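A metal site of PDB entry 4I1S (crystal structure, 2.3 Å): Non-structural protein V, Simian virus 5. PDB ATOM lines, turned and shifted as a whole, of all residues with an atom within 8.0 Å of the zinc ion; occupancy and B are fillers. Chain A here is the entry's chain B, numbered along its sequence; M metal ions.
N of Ser 26 lies close to SG of Cys 44.
The side-chain sulfur (SG) of Cys 27 sits close to the backbone NH (N) of Thr 40 (3.3 Å).
The side-chain sulfur (SG) of Cys 41 sits close to the backbone NH (N) of Gln 43 (3.4 Å).
N of Gly 2 lies close to SG of Cys 44 (3.3 Å).
SG of Cys 39 sits close to N of His 42 (3.1 Å).
The backbone carbonyl oxygen of Pro 25 lies within hydrogen-bond range of the side-chain hydroxyl of Ser 28 (2.5 Å).
The zinc ion is bound by SG of Cys 44, 2.3 Å away.
SG of Cys 27 binds the zinc ion.
The zinc ion is bound by SG of Cys 39, at 2.4 Å.
SG of Cys 41 is bound to the zinc ion, 2.4 Å away.
The zinc ion has four donor atoms within binding distance.
Residues that only touch the zinc ion: Pro 25.
Of the 17 residues printed, 5 come within 4 Å of the zinc ion.
The nearest printed residue that does not touch the zinc ion is His 42 (4.004 Å).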
ATOM      1  N   GLY A   1      29.089 -18.281 -10.280  1.00  0.00           N
ATOM      2  CA  GLY A   1      28.884 -19.674  -9.930  1.00  0.00           C
ATOM      3  C   GLY A   1      29.543 -20.072  -8.617  1.00  0.00           C
ATOM      4  O   GLY A   1      30.122 -19.218  -7.948  1.00  0.00           O
ATOM      5  N   GLY A   2      29.445 -21.350  -8.255  1.00  0.00           N
ATOM      6  CA  GLY A   2      30.154 -21.867  -7.099  1.00  0.00           C
ATOM      7  C   GLY A   2      29.383 -22.670  -6.065  1.00  0.00           C
ATOM      8  O   GLY A   2      29.988 -23.415  -5.295  1.00  0.00           O
ATOM      9  N   PHE A   3      28.055 -22.518  -6.032  1.00  0.00           N
ATOM     10  CA  PHE A   3      27.239 -23.210  -5.031  1.00  0.00           C
ATOM     11  C   PHE A   3      25.831 -23.591  -5.534  1.00  0.00           C
ATOM     12  O   PHE A   3      25.521 -23.463  -6.714  1.00  0.00           O
ATOM     13  CB  PHE A   3      27.165 -22.395  -3.739  1.00  0.00           C
ATOM     14  CG  PHE A   3      26.569 -21.009  -3.920  1.00  0.00           C
ATOM     15  CD1 PHE A   3      27.366 -19.949  -4.355  1.00  0.00           C
ATOM     16  CD2 PHE A   3      25.228 -20.778  -3.649  1.00  0.00           C
ATOM     17  CE1 PHE A   3      26.823 -18.675  -4.535  1.00  0.00           C
ATOM     18  CE2 PHE A   3      24.676 -19.505  -3.829  1.00  0.00           C
ATOM     19  CZ  PHE A   3      25.473 -18.449  -4.274  1.00  0.00           C
ATOM     20  N   HIS A   4      24.998 -24.085  -4.631  1.00  0.00           N
ATOM     21  CA  HIS A   4      23.606 -24.395  -4.957  1.00  0.00           C
ATOM     22  C   HIS A   4      22.672 -23.312  -4.438  1.00  0.00           C
ATOM     23  O   HIS A   4      22.702 -22.958  -3.256  1.00  0.00           O
ATOM     24  CB  HIS A   4      23.138 -25.723  -4.347  1.00  0.00           C
ATOM     25  CG  HIS A   4      23.442 -26.920  -5.198  1.00  0.00           C
ATOM     26  ND1 HIS A   4      22.967 -28.170  -4.887  1.00  0.00           N
ATOM     27  CD2 HIS A   4      24.164 -27.059  -6.331  1.00  0.00           C
ATOM     28  CE1 HIS A   4      23.391 -29.040  -5.798  1.00  0.00           C
ATOM     29  NE2 HIS A   4      24.124 -28.387  -6.678  1.00  0.00           N
ATOM     30  N   ASN A  24      19.265 -25.238  -7.911  1.00  0.00           N
ATOM     31  CA  ASN A  24      19.860 -24.779  -9.159  1.00  0.00           C
ATOM     32  C   ASN A  24      21.330 -24.456  -8.911  1.00  0.00           C
ATOM     33  O   ASN A  24      21.713 -24.128  -7.776  1.00  0.00           O
ATOM     34  CB  ASN A  24      19.142 -23.549  -9.700  1.00  0.00           C
ATOM     35  CG  ASN A  24      18.030 -23.902 -10.679  1.00  0.00           C
ATOM     36  OD1 ASN A  24      18.122 -24.899 -11.387  1.00  0.00           O
ATOM     37  ND2 ASN A  24      16.984 -23.091 -10.712  1.00  0.00           N
ATOM     38  N   PRO A  25      22.160 -24.559  -9.959  1.00  0.00           N
ATOM     39  CA  PRO A  25      23.549 -24.110  -9.859  1.00  0.00           C
ATOM     40  C   PRO A  25      23.570 -22.585  -9.695  1.00  0.00           C
ATOM     41  O   PRO A  25      22.737 -21.922 -10.321  1.00  0.00           O
ATOM     42  CB  PRO A  25      24.155 -24.499 -11.208  1.00  0.00           C
ATOM     43  CG  PRO A  25      23.175 -25.451 -11.825  1.00  0.00           C
ATOM     44  CD  PRO A  25      21.835 -25.087 -11.295  1.00  0.00           C
ATOM     45  N   SER A  26      24.483 -22.038  -8.902  1.00  0.00           N
ATOM     46  CA  SER A  26      24.481 -20.617  -8.581  1.00  0.00           C
ATOM     47  C   SER A  26      24.796 -19.751  -9.798  1.00  0.00           C
ATOM     48  O   SER A  26      24.598 -18.527  -9.780  1.00  0.00           O
ATOM     49  CB  SER A  26      25.471 -20.307  -7.449  1.00  0.00           C
ATOM     50  OG  SER A  26      26.789 -20.693  -7.778  1.00  0.00           O
ATOM     51  N   CYS A  27      25.268 -20.392 -10.860  1.00  0.00           N
ATOM     52  CA  CYS A  27      25.605 -19.703 -12.095  1.00  0.00           C
ATOM     53  C   CYS A  27      24.371 -19.535 -12.998  1.00  0.00           C
ATOM     54  O   CYS A  27      24.401 -18.755 -13.952  1.00  0.00           O
ATOM     55  CB  CYS A  27      26.696 -20.477 -12.847  1.00  0.00           C
ATOM     56  SG  CYS A  27      26.226 -22.133 -13.418  1.00  0.00           S
ATOM     57  N   SER A  28      23.310 -20.281 -12.721  1.00  0.00           N
ATOM     58  CA  SER A  28      22.150 -20.300 -13.604  1.00  0.00           C
ATOM     59  C   SER A  28      21.259 -19.064 -13.401  1.00  0.00           C
ATOM     60  O   SER A  28      21.357 -18.393 -12.372  1.00  0.00           O
ATOM     61  CB  SER A  28      21.355 -21.593 -13.379  1.00  0.00           C
ATOM     62  OG  SER A  28      20.888 -21.679 -12.048  1.00  0.00           O
ATOM     63  N   GLU A  38      21.083 -26.383 -15.859  1.00  0.00           N
ATOM     64  CA  GLU A  38      22.369 -27.079 -15.748  1.00  0.00           C
ATOM     65  C   GLU A  38      23.490 -26.055 -15.552  1.00  0.00           C
ATOM     66  O   GLU A  38      23.329 -24.884 -15.878  1.00  0.00           O
ATOM     67  N   CYS A  39      24.616 -26.495 -15.007  1.00  0.00           N
ATOM     68  CA  CYS A  39      25.715 -25.585 -14.650  1.00  0.00           C
ATOM     69  C   CYS A  39      26.587 -25.234 -15.851  1.00  0.00           C
ATOM     70  O   CYS A  39      27.037 -26.114 -16.574  1.00  0.00           O
ATOM     71  CB  CYS A  39      26.566 -26.215 -13.554  1.00  0.00           C
ATOM     72  SG  CYS A  39      28.151 -25.421 -13.272  1.00  0.00           S
ATOM     73  N   THR A  40      26.839 -23.949 -16.051  1.00  0.00           N
ATOM     74  CA  THR A  40      27.671 -23.502 -17.161  1.00  0.00           C
ATOM     75  C   THR A  40      29.042 -22.982 -16.702  1.00  0.00           C
ATOM     76  O   THR A  40      29.977 -22.897 -17.499  1.00  0.00           O
ATOM     77  CB  THR A  40      26.967 -22.457 -18.017  1.00  0.00           C
ATOM     78  OG1 THR A  40      26.716 -21.284 -17.219  1.00  0.00           O
ATOM     79  CG2 THR A  40      25.628 -22.996 -18.532  1.00  0.00           C
ATOM     80  N   CYS A  41      29.170 -22.671 -15.415  1.00  0.00           N
ATOM     81  CA  CYS A  41      30.410 -22.143 -14.865  1.00  0.00           C
ATOM     82  C   CYS A  41      31.400 -23.239 -14.488  1.00  0.00           C
ATOM     83  O   CYS A  41      32.583 -22.972 -14.257  1.00  0.00           O
ATOM     84  CB  CYS A  41      30.146 -21.271 -13.642  1.00  0.00           C
ATOM     85  SG  CYS A  41      29.840 -22.228 -12.132  1.00  0.00           S
ATOM     86  N   HIS A  42      30.897 -24.474 -14.408  1.00  0.00           N
ATOM     87  CA  HIS A  42      31.723 -25.659 -14.150  1.00  0.00           C
ATOM     88  C   HIS A  42      32.363 -25.727 -12.760  1.00  0.00           C
ATOM     89  O   HIS A  42      33.100 -26.669 -12.458  1.00  0.00           O
ATOM     90  CB  HIS A  42      32.784 -25.843 -15.237  1.00  0.00           C
ATOM     91  CG  HIS A  42      32.214 -25.938 -16.626  1.00  0.00           C
ATOM     92  ND1 HIS A  42      31.260 -26.878 -16.969  1.00  0.00           N
ATOM     93  CD2 HIS A  42      32.458 -25.217 -17.746  1.00  0.00           C
ATOM     94  CE1 HIS A  42      30.946 -26.732 -18.242  1.00  0.00           C
ATOM     95  NE2 HIS A  42      31.658 -25.736 -18.730  1.00  0.00           N
ATOM     96  N   GLN A  43      32.084 -24.734 -11.916  1.00  0.00           N
ATOM     97  CA  GLN A  43      32.587 -24.753 -10.548  1.00  0.00           C
ATOM     98  C   GLN A  43      31.518 -25.186  -9.545  1.00  0.00           C
ATOM     99  O   GLN A  43      31.817 -25.392  -8.367  1.00  0.00           O
ATOM    100  CB  GLN A  43      33.168 -23.392 -10.161  1.00  0.00           C
ATOM    101  N   CYS A  44      30.272 -25.315 -10.013  1.00  0.00           N
ATOM    102  CA  CYS A  44      29.165 -25.717  -9.140  1.00  0.00           C
ATOM    103  C   CYS A  44      29.163 -27.216  -8.852  1.00  0.00           C
ATOM    104  O   CYS A  44      29.308 -28.034  -9.756  1.00  0.00           O
ATOM    105  CB  CYS A  44      27.810 -25.317  -9.739  1.00  0.00           C
ATOM    106  SG  CYS A  44      27.559 -23.540  -9.946  1.00  0.00           S
ATOM    107  N   PRO A  45      28.981 -27.584  -7.567  1.00  0.00           N
ATOM    108  CA  PRO A  45      28.920 -28.977  -7.096  1.00  0.00           C
ATOM    109  C   PRO A  45      27.739 -29.753  -7.667  1.00  0.00           C
ATOM    110  O   PRO A  45      26.796 -29.150  -8.186  1.00  0.00           O
ATOM    111  CB  PRO A  45      28.772 -28.830  -5.580  1.00  0.00           C
ATOM    112  CG  PRO A  45      28.227 -27.445  -5.363  1.00  0.00           C
ATOM    113  CD  PRO A  45      28.853 -26.621  -6.461  1.00  0.00           C
HETATM  114 ZN    ZN M   1      27.758 -23.356 -12.188  1.00  0.00          ZN
